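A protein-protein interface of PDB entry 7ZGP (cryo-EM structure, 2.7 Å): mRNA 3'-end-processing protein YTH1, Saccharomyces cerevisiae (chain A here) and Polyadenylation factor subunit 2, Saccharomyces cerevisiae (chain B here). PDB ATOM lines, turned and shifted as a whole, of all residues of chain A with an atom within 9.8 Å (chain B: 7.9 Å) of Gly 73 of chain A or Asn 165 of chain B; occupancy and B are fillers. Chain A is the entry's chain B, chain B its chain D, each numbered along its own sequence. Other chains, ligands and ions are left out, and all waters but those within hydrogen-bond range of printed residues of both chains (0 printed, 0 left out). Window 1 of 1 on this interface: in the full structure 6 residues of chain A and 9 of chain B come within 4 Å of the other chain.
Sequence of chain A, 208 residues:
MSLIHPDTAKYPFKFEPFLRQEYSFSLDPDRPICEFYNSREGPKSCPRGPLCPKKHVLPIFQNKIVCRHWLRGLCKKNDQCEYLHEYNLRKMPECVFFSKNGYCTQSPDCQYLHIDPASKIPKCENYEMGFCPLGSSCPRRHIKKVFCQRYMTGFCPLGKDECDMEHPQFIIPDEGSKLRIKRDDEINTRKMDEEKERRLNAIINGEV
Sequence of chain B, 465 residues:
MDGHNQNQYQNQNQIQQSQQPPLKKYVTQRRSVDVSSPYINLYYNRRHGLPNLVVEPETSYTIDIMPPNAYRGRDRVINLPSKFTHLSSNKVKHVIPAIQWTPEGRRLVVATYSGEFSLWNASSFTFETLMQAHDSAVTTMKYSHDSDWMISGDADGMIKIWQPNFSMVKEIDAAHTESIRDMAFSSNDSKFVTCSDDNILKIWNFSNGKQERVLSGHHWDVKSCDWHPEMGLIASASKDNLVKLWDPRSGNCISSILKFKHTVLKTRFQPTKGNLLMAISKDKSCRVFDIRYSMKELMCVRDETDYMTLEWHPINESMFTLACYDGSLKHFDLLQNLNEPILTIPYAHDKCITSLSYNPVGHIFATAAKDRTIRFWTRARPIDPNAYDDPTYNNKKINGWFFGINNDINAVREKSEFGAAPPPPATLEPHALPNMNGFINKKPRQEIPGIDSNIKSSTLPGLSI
O of Arg 72 of chain A lies within hydrogen-bond range of NH2 of Arg 107 of chain B, at 2.6 Å.
The side-chain sulfur (SD) of Met 131 of chain B sits at hydrogen-bond distance from the side-chain amino group (NZ) of Lys 76 of chain A, at 3.1 Å.
O of Phe 166 of chain B is in hydrogen-bond range of NZ of Lys 76 of chain A, at 2.5 Å.
O of Lys 76 of chain A lies close to OG of Ser 167 of chain B, at 3.3 Å.
ND2 of Asn 165 of chain B sits at hydrogen-bond distance from OD1 of Asn 78 of chain A (2.7 Å).
The backbone carbonyl oxygen (O) of Cys 75 of chain A sits close to the side-chain amide nitrogen (ND2) of Asn 165 of chain B, 2.3 Å away.
O of His 69 of chain A sits at hydrogen-bond distance from N of Leu 74 of chain A.
The backbone carbonyl oxygen (O) of His 69 of chain A is in hydrogen-bond range of the backbone NH (N) of Cys 75 of chain A.
The side-chain sulfur (SG) of Cys 75 of chain A lies close to the backbone NH (N) of Lys 77 of chain A (3.7 Å).
The side-chain sulfur of Cys 75 of chain A sits close to the backbone NH of Asn 78 of chain A, at 3.7 Å.
OD1 of Asn 165 of chain B lies close to OE1 of Gln 163 of chain B (3.5 Å).
The side-chain amide nitrogen (ND2) of Asn 165 of chain B is in hydrogen-bond range of the side-chain hydroxyl (OG) of Ser 167 of chain B, 2.8 Å away.
Among the printed residues, merely in contact across the chains: Arg 72 of chain A with Arg 106 of chain B (3.6 Å), Gly 73 of chain A with Asn 165 of chain B (3.8 Å), Leu 74 of chain A with Arg 107 of chain B (3.8 Å), Leu 74 of chain A with Leu 119 of chain B (3.7 Å), Leu 74 of chain A with Phe 166 of chain B (3.6 Å), Cys 75 of chain A with Ser 167 of chain B (3.8 Å), Lys 76 of chain A with Asn 165 of chain B (3.9 Å) and Asn 78 of chain A with Gln 163 of chain B (3.8 Å).
Among the printed residues, 14 pairs touch across the chains.
Among the printed residues, no Asp or Glu carboxylate lies within 4 Å of a Lys or Arg side-chain nitrogen of the other chain.
Gly 73 of chain A touches just one residue of chain B: Asn 165 (3.8 Å).
Printed residues of chain B within 4 Å of Lys 76 of chain A: Met 131, Asn 165, Phe 166 and Ser 167.
Of the printed residues of chain A, Arg 107 of chain B touches Arg 72 and Leu 74.
Of the printed residues of chain A, Met 131 of chain B touches Lys 76 (3.1 Å).
Ser 147 of chain B touches none of the printed residues of chain A.
Gln 163 of chain B touches just one residue of chain A: Asn 78 (3.8 Å).
No residue of chain A comes within 4 Å of Pro 164 of chain B.
Of chain A, only Cys 75 and Lys 76 come within 4 Å of Ser 167 of chain B.
The nearest residue of chain A that does not touch Asn 165 of chain B is Leu 74 of chain A (4.04 Å).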
ATOM      1  N   VAL A  66       2.399 -27.005   5.291  1.00  0.00           N
ATOM      2  CA  VAL A  66       3.621 -26.229   5.131  1.00  0.00           C
ATOM      3  C   VAL A  66       4.346 -26.661   3.866  1.00  0.00           C
ATOM      4  O   VAL A  66       4.485 -27.858   3.586  1.00  0.00           O
ATOM      5  CB  VAL A  66       4.514 -26.388   6.370  1.00  0.00           C
ATOM      6  CG1 VAL A  66       5.804 -25.601   6.208  1.00  0.00           C
ATOM      7  CG2 VAL A  66       3.768 -25.944   7.614  1.00  0.00           C
ATOM      8  N   CYS A  67       4.813 -25.682   3.095  1.00  0.00           N
ATOM      9  CA  CYS A  67       5.540 -25.969   1.866  1.00  0.00           C
ATOM     10  C   CYS A  67       6.898 -26.579   2.186  1.00  0.00           C
ATOM     11  O   CYS A  67       7.706 -25.977   2.897  1.00  0.00           O
ATOM     12  CB  CYS A  67       5.707 -24.690   1.049  1.00  0.00           C
ATOM     13  SG  CYS A  67       6.692 -24.879  -0.450  1.00  0.00           S
ATOM     14  N   ARG A  68       7.147 -27.778   1.655  1.00  0.00           N
ATOM     15  CA  ARG A  68       8.414 -28.451   1.917  1.00  0.00           C
ATOM     16  C   ARG A  68       9.585 -27.721   1.271  1.00  0.00           C
ATOM     17  O   ARG A  68      10.702 -27.758   1.800  1.00  0.00           O
ATOM     18  CB  ARG A  68       8.348 -29.903   1.436  1.00  0.00           C
ATOM     19  CG  ARG A  68       8.428 -30.080  -0.072  1.00  0.00           C
ATOM     20  CD  ARG A  68       8.471 -31.549  -0.453  1.00  0.00           C
ATOM     21  NE  ARG A  68       7.143 -32.154  -0.449  1.00  0.00           N
ATOM     22  CZ  ARG A  68       6.698 -32.977   0.490  1.00  0.00           C
ATOM     23  NH1 ARG A  68       7.450 -33.318   1.523  1.00  0.00           N
ATOM     24  NH2 ARG A  68       5.466 -33.469   0.390  1.00  0.00           N
ATOM     25  N   HIS A  69       9.357 -27.057   0.137  1.00  0.00           N
ATOM     26  CA  HIS A  69      10.423 -26.311  -0.518  1.00  0.00           C
ATOM     27  C   HIS A  69      10.705 -24.989   0.179  1.00  0.00           C
ATOM     28  O   HIS A  69      11.841 -24.504   0.141  1.00  0.00           O
ATOM     29  CB  HIS A  69      10.068 -26.074  -1.985  1.00  0.00           C
ATOM     30  CG  HIS A  69       9.624 -27.310  -2.703  1.00  0.00           C
ATOM     31  ND1 HIS A  69       8.302 -27.689  -2.780  1.00  0.00           N
ATOM     32  CD2 HIS A  69      10.327 -28.256  -3.367  1.00  0.00           C
ATOM     33  CE1 HIS A  69       8.210 -28.815  -3.465  1.00  0.00           C
ATOM     34  NE2 HIS A  69       9.424 -29.181  -3.833  1.00  0.00           N
ATOM     35  N   TRP A  70       9.692 -24.393   0.808  1.00  0.00           N
ATOM     36  CA  TRP A  70       9.906 -23.166   1.566  1.00  0.00           C
ATOM     37  C   TRP A  70      10.803 -23.409   2.774  1.00  0.00           C
ATOM     38  O   TRP A  70      11.625 -22.555   3.123  1.00  0.00           O
ATOM     39  CB  TRP A  70       8.564 -22.580   2.000  1.00  0.00           C
ATOM     40  CG  TRP A  70       8.690 -21.348   2.834  1.00  0.00           C
ATOM     41  CD1 TRP A  70       8.982 -20.089   2.399  1.00  0.00           C
ATOM     42  CD2 TRP A  70       8.521 -21.253   4.251  1.00  0.00           C
ATOM     43  NE1 TRP A  70       9.010 -19.218   3.458  1.00  0.00           N
ATOM     44  CE2 TRP A  70       8.731 -19.908   4.607  1.00  0.00           C
ATOM     45  CE3 TRP A  70       8.217 -22.177   5.255  1.00  0.00           C
ATOM     46  CZ2 TRP A  70       8.645 -19.463   5.922  1.00  0.00           C
ATOM     47  CZ3 TRP A  70       8.132 -21.733   6.559  1.00  0.00           C
ATOM     48  CH2 TRP A  70       8.343 -20.388   6.881  1.00  0.00           C
ATOM     49  N   LEU A  71      10.653 -24.564   3.427  1.00  0.00           N
ATOM     50  CA  LEU A  71      11.477 -24.870   4.592  1.00  0.00           C
ATOM     51  C   LEU A  71      12.952 -24.961   4.229  1.00  0.00           C
ATOM     52  O   LEU A  71      13.814 -24.642   5.055  1.00  0.00           O
ATOM     53  CB  LEU A  71      11.009 -26.173   5.235  1.00  0.00           C
ATOM     54  CG  LEU A  71       9.586 -26.165   5.791  1.00  0.00           C
ATOM     55  CD1 LEU A  71       9.146 -27.573   6.138  1.00  0.00           C
ATOM     56  CD2 LEU A  71       9.492 -25.259   7.005  1.00  0.00           C
ATOM     57  N   ARG A  72      13.261 -25.393   3.012  1.00  0.00           N
ATOM     58  CA  ARG A  72      14.631 -25.437   2.523  1.00  0.00           C
ATOM     59  C   ARG A  72      15.054 -24.140   1.851  1.00  0.00           C
ATOM     60  O   ARG A  72      16.179 -24.056   1.351  1.00  0.00           O
ATOM     61  CB  ARG A  72      14.802 -26.600   1.542  1.00  0.00           C
ATOM     62  CG  ARG A  72      14.236 -27.918   2.038  1.00  0.00           C
ATOM     63  CD  ARG A  72      15.007 -28.433   3.240  1.00  0.00           C
ATOM     64  NE  ARG A  72      16.440 -28.483   2.982  1.00  0.00           N
ATOM     65  CZ  ARG A  72      17.374 -28.205   3.880  1.00  0.00           C
ATOM     66  NH1 ARG A  72      17.062 -27.855   5.117  1.00  0.00           N
ATOM     67  NH2 ARG A  72      18.655 -28.280   3.529  1.00  0.00           N
ATOM     68  N   GLY A  73      14.186 -23.134   1.831  1.00  0.00           N
ATOM     69  CA  GLY A  73      14.473 -21.897   1.129  1.00  0.00           C
ATOM     70  C   GLY A  73      14.559 -22.067  -0.371  1.00  0.00           C
ATOM     71  O   GLY A  73      15.364 -21.391  -1.022  1.00  0.00           O
ATOM     72  N   LEU A  74      13.744 -22.954  -0.937  1.00  0.00           N
ATOM     73  CA  LEU A  74      13.804 -23.272  -2.359  1.00  0.00           C
ATOM     74  C   LEU A  74      12.405 -23.339  -2.954  1.00  0.00           C
ATOM     75  O   LEU A  74      12.117 -24.187  -3.806  1.00  0.00           O
ATOM     76  CB  LEU A  74      14.549 -24.585  -2.594  1.00  0.00           C
ATOM     77  CG  LEU A  74      16.036 -24.592  -2.247  1.00  0.00           C
ATOM     78  CD1 LEU A  74      16.581 -26.009  -2.267  1.00  0.00           C
ATOM     79  CD2 LEU A  74      16.809 -23.704  -3.202  1.00  0.00           C
ATOM     80  N   CYS A  75      11.518 -22.448  -2.523  1.00  0.00           N
ATOM     81  CA  CYS A  75      10.165 -22.386  -3.064  1.00  0.00           C
ATOM     82  C   CYS A  75      10.159 -21.464  -4.276  1.00  0.00           C
ATOM     83  O   CYS A  75      10.458 -20.271  -4.156  1.00  0.00           O
ATOM     84  CB  CYS A  75       9.175 -21.894  -2.010  1.00  0.00           C
ATOM     85  SG  CYS A  75       7.465 -21.812  -2.587  1.00  0.00           S
ATOM     86  N   LYS A  76       9.813 -22.015  -5.439  1.00  0.00           N
ATOM     87  CA  LYS A  76       9.813 -21.242  -6.673  1.00  0.00           C
ATOM     88  C   LYS A  76       8.533 -20.448  -6.886  1.00  0.00           C
ATOM     89  O   LYS A  76       8.491 -19.607  -7.790  1.00  0.00           O
ATOM     90  CB  LYS A  76      10.042 -22.166  -7.871  1.00  0.00           C
ATOM     91  CG  LYS A  76      11.434 -22.766  -7.933  1.00  0.00           C
ATOM     92  CD  LYS A  76      11.543 -23.787  -9.052  1.00  0.00           C
ATOM     93  CE  LYS A  76      12.716 -24.722  -8.834  1.00  0.00           C
ATOM     94  NZ  LYS A  76      14.009 -23.995  -8.867  1.00  0.00           N
ATOM     95  N   LYS A  77       7.495 -20.685  -6.086  1.00  0.00           N
ATOM     96  CA  LYS A  77       6.216 -20.020  -6.281  1.00  0.00           C
ATOM     97  C   LYS A  77       6.033 -18.784  -5.411  1.00  0.00           C
ATOM     98  O   LYS A  77       5.189 -17.942  -5.738  1.00  0.00           O
ATOM     99  CB  LYS A  77       5.071 -21.001  -6.016  1.00  0.00           C
ATOM    100  CG  LYS A  77       5.082 -22.209  -6.933  1.00  0.00           C
ATOM    101  CD  LYS A  77       3.995 -23.194  -6.561  1.00  0.00           C
ATOM    102  CE  LYS A  77       4.108 -24.469  -7.378  1.00  0.00           C
ATOM    103  NZ  LYS A  77       3.247 -25.552  -6.833  1.00  0.00           N
ATOM    104  N   ASN A  78       6.793 -18.659  -4.327  1.00  0.00           N
ATOM    105  CA  ASN A  78       6.777 -17.481  -3.447  1.00  0.00           C
ATOM    106  C   ASN A  78       5.360 -17.323  -2.899  1.00  0.00           C
ATOM    107  O   ASN A  78       4.773 -18.319  -2.447  1.00  0.00           O
ATOM    108  CB  ASN A  78       7.330 -16.280  -4.205  1.00  0.00           C
ATOM    109  CG  ASN A  78       8.688 -16.556  -4.817  1.00  0.00           C
ATOM    110  OD1 ASN A  78       9.650 -16.854  -4.111  1.00  0.00           O
ATOM    111  ND2 ASN A  78       8.771 -16.461  -6.138  1.00  0.00           N
ATOM    112  N   ASP A  79       4.776 -16.123  -2.916  1.00  0.00           N
ATOM    113  CA  ASP A  79       3.451 -15.908  -2.348  1.00  0.00           C
ATOM    114  C   ASP A  79       2.343 -16.579  -3.148  1.00  0.00           C
ATOM    115  O   ASP A  79       1.219 -16.685  -2.643  1.00  0.00           O
ATOM    116  CB  ASP A  79       3.169 -14.409  -2.238  1.00  0.00           C
ATOM    117  CG  ASP A  79       4.236 -13.674  -1.452  1.00  0.00           C
ATOM    118  OD1 ASP A  79       4.322 -13.883  -0.225  1.00  0.00           O
ATOM    119  OD2 ASP A  79       4.989 -12.887  -2.064  1.00  0.00           O
ATOM    120  N   GLN A  80       2.622 -17.029  -4.368  1.00  0.00           N
ATOM    121  CA  GLN A  80       1.625 -17.717  -5.176  1.00  0.00           C
ATOM    122  C   GLN A  80       1.559 -19.210  -4.883  1.00  0.00           C
ATOM    123  O   GLN A  80       0.764 -19.913  -5.515  1.00  0.00           O
ATOM    124  CB  GLN A  80       1.908 -17.496  -6.663  1.00  0.00           C
ATOM    125  CG  GLN A  80       2.496 -16.135  -6.995  1.00  0.00           C
ATOM    126  CD  GLN A  80       1.653 -14.990  -6.472  1.00  0.00           C
ATOM    127  OE1 GLN A  80       0.450 -14.923  -6.725  1.00  0.00           O
ATOM    128  NE2 GLN A  80       2.282 -14.078  -5.740  1.00  0.00           N
ATOM    129  N   CYS A  81       2.372 -19.703  -3.952  1.00  0.00           N
ATOM    130  CA  CYS A  81       2.372 -21.120  -3.621  1.00  0.00           C
ATOM    131  C   CYS A  81       1.036 -21.530  -3.012  1.00  0.00           C
ATOM    132  O   CYS A  81       0.385 -20.757  -2.305  1.00  0.00           O
ATOM    133  CB  CYS A  81       3.512 -21.434  -2.652  1.00  0.00           C
ATOM    134  SG  CYS A  81       3.867 -23.190  -2.436  1.00  0.00           S
ATOM    135  N   HIS A  85       3.415 -21.083   3.757  1.00  0.00           N
ATOM    136  CA  HIS A  85       4.754 -20.528   3.935  1.00  0.00           C
ATOM    137  C   HIS A  85       4.954 -19.993   5.344  1.00  0.00           C
ATOM    138  O   HIS A  85       5.625 -18.979   5.552  1.00  0.00           O
ATOM    139  CB  HIS A  85       5.026 -19.441   2.900  1.00  0.00           C
ATOM    140  CG  HIS A  85       5.508 -19.972   1.588  1.00  0.00           C
ATOM    141  ND1 HIS A  85       6.211 -19.202   0.686  1.00  0.00           N
ATOM    142  CD2 HIS A  85       5.390 -21.197   1.025  1.00  0.00           C
ATOM    143  CE1 HIS A  85       6.505 -19.931  -0.376  1.00  0.00           C
ATOM    144  NE2 HIS A  85       6.017 -21.145  -0.195  1.00  0.00           N
ATOM    145  N   ARG B 106      26.004 -21.789   1.827  1.00  0.00           N
ATOM    146  CA  ARG B 106      25.143 -22.845   2.350  1.00  0.00           C
ATOM    147  C   ARG B 106      25.121 -24.056   1.427  1.00  0.00           C
ATOM    148  O   ARG B 106      25.151 -25.200   1.894  1.00  0.00           O
ATOM    149  CB  ARG B 106      23.729 -22.312   2.561  1.00  0.00           C
ATOM    150  CG  ARG B 106      22.735 -23.370   2.998  1.00  0.00           C
ATOM    151  CD  ARG B 106      21.317 -22.847   2.949  1.00  0.00           C
ATOM    152  NE  ARG B 106      20.378 -23.767   3.578  1.00  0.00           N
ATOM    153  CZ  ARG B 106      19.100 -23.496   3.796  1.00  0.00           C
ATOM    154  NH1 ARG B 106      18.572 -22.334   3.452  1.00  0.00           N
ATOM    155  NH2 ARG B 106      18.333 -24.414   4.374  1.00  0.00           N
ATOM    156  N   ARG B 107      25.062 -23.829   0.120  1.00  0.00           N
ATOM    157  CA  ARG B 107      24.934 -24.902  -0.851  1.00  0.00           C
ATOM    158  C   ARG B 107      25.906 -24.683  -1.999  1.00  0.00           C
ATOM    159  O   ARG B 107      26.371 -23.569  -2.247  1.00  0.00           O
ATOM    160  CB  ARG B 107      23.507 -25.003  -1.401  1.00  0.00           C
ATOM    161  CG  ARG B 107      22.465 -25.357  -0.364  1.00  0.00           C
ATOM    162  CD  ARG B 107      21.188 -25.830  -1.021  1.00  0.00           C
ATOM    163  NE  ARG B 107      20.134 -26.063  -0.044  1.00  0.00           N
ATOM    164  CZ  ARG B 107      19.227 -25.162   0.303  1.00  0.00           C
ATOM    165  NH1 ARG B 107      19.223 -23.947  -0.220  1.00  0.00           N
ATOM    166  NH2 ARG B 107      18.300 -25.487   1.201  1.00  0.00           N
ATOM    167  N   LEU B 119      21.862 -29.130  -6.390  1.00  0.00           N
ATOM    168  CA  LEU B 119      22.328 -28.480  -5.178  1.00  0.00           C
ATOM    169  C   LEU B 119      22.964 -29.504  -4.250  1.00  0.00           C
ATOM    170  O   LEU B 119      22.635 -30.691  -4.290  1.00  0.00           O
ATOM    171  CB  LEU B 119      21.177 -27.765  -4.473  1.00  0.00           C
ATOM    172  CG  LEU B 119      20.481 -26.707  -5.326  1.00  0.00           C
ATOM    173  CD1 LEU B 119      19.469 -25.938  -4.505  1.00  0.00           C
ATOM    174  CD2 LEU B 119      21.502 -25.766  -5.934  1.00  0.00           C
ATOM    175  N   MET B 131      17.081 -29.792 -11.059  1.00  0.00           N
ATOM    176  CA  MET B 131      16.281 -28.622 -11.398  1.00  0.00           C
ATOM    177  C   MET B 131      15.990 -28.448 -12.881  1.00  0.00           C
ATOM    178  O   MET B 131      14.956 -27.851 -13.209  1.00  0.00           O
ATOM    179  CB  MET B 131      16.964 -27.344 -10.889  1.00  0.00           C
ATOM    180  CG  MET B 131      16.002 -26.310 -10.345  1.00  0.00           C
ATOM    181  SD  MET B 131      16.704 -25.431  -8.942  1.00  0.00           S
ATOM    182  CE  MET B 131      16.636 -26.707  -7.687  1.00  0.00           C
ATOM    183  N   TYR B 143      26.788 -15.590  -9.076  1.00  0.00           N
ATOM    184  CA  TYR B 143      25.819 -14.948  -8.151  1.00  0.00           C
ATOM    185  C   TYR B 143      26.130 -13.454  -8.054  1.00  0.00           C
ATOM    186  O   TYR B 143      27.287 -13.063  -8.298  1.00  0.00           O
ATOM    187  CB  TYR B 143      25.868 -15.605  -6.771  1.00  0.00           C
ATOM    188  CG  TYR B 143      24.934 -16.773  -6.590  1.00  0.00           C
ATOM    189  CD1 TYR B 143      23.612 -16.577  -6.224  1.00  0.00           C
ATOM    190  CD2 TYR B 143      25.368 -18.075  -6.774  1.00  0.00           C
ATOM    191  CE1 TYR B 143      22.746 -17.642  -6.050  1.00  0.00           C
ATOM    192  CE2 TYR B 143      24.515 -19.151  -6.604  1.00  0.00           C
ATOM    193  CZ  TYR B 143      23.199 -18.934  -6.241  1.00  0.00           C
ATOM    194  OH  TYR B 143      22.351 -19.989  -6.071  1.00  0.00           O
ATOM    195  N   SER B 147      24.100 -10.894  -3.427  1.00  0.00           N
ATOM    196  CA  SER B 147      23.617 -12.250  -3.055  1.00  0.00           C
ATOM    197  C   SER B 147      22.122 -12.383  -3.352  1.00  0.00           C
ATOM    198  O   SER B 147      21.486 -13.275  -2.763  1.00  0.00           O
ATOM    199  CB  SER B 147      23.906 -12.542  -1.607  1.00  0.00           C
ATOM    200  OG  SER B 147      25.279 -12.335  -1.315  1.00  0.00           O
ATOM    201  N   ASP B 148      21.586 -11.539  -4.234  1.00  0.00           N
ATOM    202  CA  ASP B 148      20.123 -11.554  -4.500  1.00  0.00           C
ATOM    203  C   ASP B 148      19.833 -12.078  -5.906  1.00  0.00           C
ATOM    204  O   ASP B 148      18.654 -12.350  -6.192  1.00  0.00           O
ATOM    205  CB  ASP B 148      19.515 -10.160  -4.336  1.00  0.00           C
ATOM    206  CG  ASP B 148      19.445  -9.703  -2.890  1.00  0.00           C
ATOM    207  OD1 ASP B 148      20.017 -10.396  -2.027  1.00  0.00           O
ATOM    208  OD2 ASP B 148      18.813  -8.659  -2.640  1.00  0.00           O
ATOM    209  N   TRP B 149      20.856 -12.205  -6.751  1.00  0.00           N
ATOM    210  CA  TRP B 149      20.586 -12.597  -8.158  1.00  0.00           C
ATOM    211  C   TRP B 149      21.676 -13.505  -8.716  1.00  0.00           C
ATOM    212  O   TRP B 149      22.859 -13.162  -8.570  1.00  0.00           O
ATOM    213  CB  TRP B 149      20.436 -11.350  -9.039  1.00  0.00           C
ATOM    214  CG  TRP B 149      19.262 -10.485  -8.701  1.00  0.00           C
ATOM    215  CD1 TRP B 149      19.285  -9.282  -8.059  1.00  0.00           C
ATOM    216  CD2 TRP B 149      17.881 -10.755  -9.000  1.00  0.00           C
ATOM    217  NE1 TRP B 149      18.015  -8.785  -7.935  1.00  0.00           N
ATOM    218  CE2 TRP B 149      17.133  -9.666  -8.503  1.00  0.00           C
ATOM    219  CE3 TRP B 149      17.206 -11.803  -9.633  1.00  0.00           C
ATOM    220  CZ2 TRP B 149      15.746  -9.602  -8.622  1.00  0.00           C
ATOM    221  CZ3 TRP B 149      15.836 -11.738  -9.749  1.00  0.00           C
ATOM    222  CH2 TRP B 149      15.119 -10.652  -9.250  1.00  0.00           C
ATOM    223  N   TRP B 162      18.213 -15.783 -12.160  1.00  0.00           N
ATOM    224  CA  TRP B 162      17.610 -16.604 -11.123  1.00  0.00           C
ATOM    225  C   TRP B 162      17.562 -15.847  -9.805  1.00  0.00           C
ATOM    226  O   TRP B 162      18.523 -15.169  -9.430  1.00  0.00           O
ATOM    227  CB  TRP B 162      18.388 -17.908 -10.928  1.00  0.00           C
ATOM    228  CG  TRP B 162      18.624 -18.665 -12.189  1.00  0.00           C
ATOM    229  CD1 TRP B 162      19.611 -18.448 -13.101  1.00  0.00           C
ATOM    230  CD2 TRP B 162      17.860 -19.770 -12.679  1.00  0.00           C
ATOM    231  NE1 TRP B 162      19.508 -19.347 -14.132  1.00  0.00           N
ATOM    232  CE2 TRP B 162      18.440 -20.171 -13.896  1.00  0.00           C
ATOM    233  CE3 TRP B 162      16.740 -20.459 -12.206  1.00  0.00           C
ATOM    234  CZ2 TRP B 162      17.939 -21.228 -14.646  1.00  0.00           C
ATOM    235  CZ3 TRP B 162      16.244 -21.509 -12.952  1.00  0.00           C
ATOM    236  CH2 TRP B 162      16.843 -21.883 -14.160  1.00  0.00           C
ATOM    237  N   GLN B 163      16.434 -15.966  -9.114  1.00  0.00           N
ATOM    238  CA  GLN B 163      16.348 -15.535  -7.735  1.00  0.00           C
ATOM    239  C   GLN B 163      17.075 -16.541  -6.843  1.00  0.00           C
ATOM    240  O   GLN B 163      17.324 -17.676  -7.256  1.00  0.00           O
ATOM    241  CB  GLN B 163      14.885 -15.396  -7.320  1.00  0.00           C
ATOM    242  CG  GLN B 163      14.324 -13.999  -7.491  1.00  0.00           C
ATOM    243  CD  GLN B 163      12.851 -13.919  -7.150  1.00  0.00           C
ATOM    244  OE1 GLN B 163      12.155 -14.933  -7.109  1.00  0.00           O
ATOM    245  NE2 GLN B 163      12.366 -12.709  -6.900  1.00  0.00           N
ATOM    246  N   PRO B 164      17.444 -16.146  -5.620  1.00  0.00           N
ATOM    247  CA  PRO B 164      18.175 -17.080  -4.746  1.00  0.00           C
ATOM    248  C   PRO B 164      17.410 -18.352  -4.430  1.00  0.00           C
ATOM    249  O   PRO B 164      18.036 -19.364  -4.097  1.00  0.00           O
ATOM    250  CB  PRO B 164      18.432 -16.252  -3.478  1.00  0.00           C
ATOM    251  CG  PRO B 164      17.495 -15.094  -3.563  1.00  0.00           C
ATOM    252  CD  PRO B 164      17.327 -14.811  -5.013  1.00  0.00           C
ATOM    253  N   ASN B 165      16.083 -18.340  -4.522  1.00  0.00           N
ATOM    254  CA  ASN B 165      15.295 -19.557  -4.395  1.00  0.00           C
ATOM    255  C   ASN B 165      15.204 -20.332  -5.704  1.00  0.00           C
ATOM    256  O   ASN B 165      14.380 -21.246  -5.810  1.00  0.00           O
ATOM    257  CB  ASN B 165      13.891 -19.227  -3.878  1.00  0.00           C
ATOM    258  CG  ASN B 165      13.071 -18.438  -4.877  1.00  0.00           C
ATOM    259  OD1 ASN B 165      13.612 -17.794  -5.771  1.00  0.00           O
ATOM    260  ND2 ASN B 165      11.756 -18.478  -4.721  1.00  0.00           N
ATOM    261  N   PHE B 166      16.030 -19.973  -6.689  1.00  0.00           N
ATOM    262  CA  PHE B 166      16.064 -20.630  -7.996  1.00  0.00           C
ATOM    263  C   PHE B 166      14.720 -20.523  -8.712  1.00  0.00           C
ATOM    264  O   PHE B 166      14.204 -21.491  -9.273  1.00  0.00           O
ATOM    265  CB  PHE B 166      16.514 -22.086  -7.870  1.00  0.00           C
ATOM    266  CG  PHE B 166      17.957 -22.234  -7.499  1.00  0.00           C
ATOM    267  CD1 PHE B 166      18.943 -22.152  -8.464  1.00  0.00           C
ATOM    268  CD2 PHE B 166      18.329 -22.436  -6.183  1.00  0.00           C
ATOM    269  CE1 PHE B 166      20.271 -22.280  -8.124  1.00  0.00           C
ATOM    270  CE2 PHE B 166      19.656 -22.564  -5.838  1.00  0.00           C
ATOM    271  CZ  PHE B 166      20.628 -22.484  -6.810  1.00  0.00           C
ATOM    272  N   SER B 167      14.193 -19.299  -8.773  1.00  0.00           N
ATOM    273  CA  SER B 167      12.955 -19.062  -9.554  1.00  0.00           C
ATOM    274  C   SER B 167      13.332 -18.227 -10.780  1.00  0.00           C
ATOM    275  O   SER B 167      13.516 -17.011 -10.616  1.00  0.00           O
ATOM    276  CB  SER B 167      11.923 -18.359  -8.726  1.00  0.00           C
ATOM    277  OG  SER B 167      11.743 -19.018  -7.483  1.00  0.00           O
ATOM    278  N   MET B 168      13.479 -18.858 -11.948  1.00  0.00           N
ATOM    279  CA  MET B 168      13.914 -18.116 -13.163  1.00  0.00           C
ATOM    280  C   MET B 168      12.964 -16.932 -13.363  1.00  0.00           C
ATOM    281  O   MET B 168      11.747 -17.173 -13.433  1.00  0.00           O
ATOM    282  CB  MET B 168      13.899 -19.022 -14.396  1.00  0.00           C
ATOM    283  CG  MET B 168      14.779 -18.522 -15.522  1.00  0.00           C
ATOM    284  SD  MET B 168      13.830 -17.630 -16.774  1.00  0.00           S
ATOM    285  CE  MET B 168      12.687 -18.912 -17.283  1.00  0.00           C
ATOM    286  N   VAL B 169      13.497 -15.712 -13.467  1.00  0.00           N
ATOM    287  CA  VAL B 169      12.620 -14.504 -13.531  1.00  0.00           C
ATOM    288  C   VAL B 169      12.782 -13.791 -14.873  1.00  0.00           C
ATOM    289  O   VAL B 169      11.903 -12.974 -15.201  1.00  0.00           O
ATOM    290  CB  VAL B 169      12.945 -13.546 -12.368  1.00  0.00           C
ATOM    291  CG1 VAL B 169      12.639 -14.166 -11.015  1.00  0.00           C
ATOM    292  CG2 VAL B 169      14.388 -13.072 -12.423  1.00  0.00           C
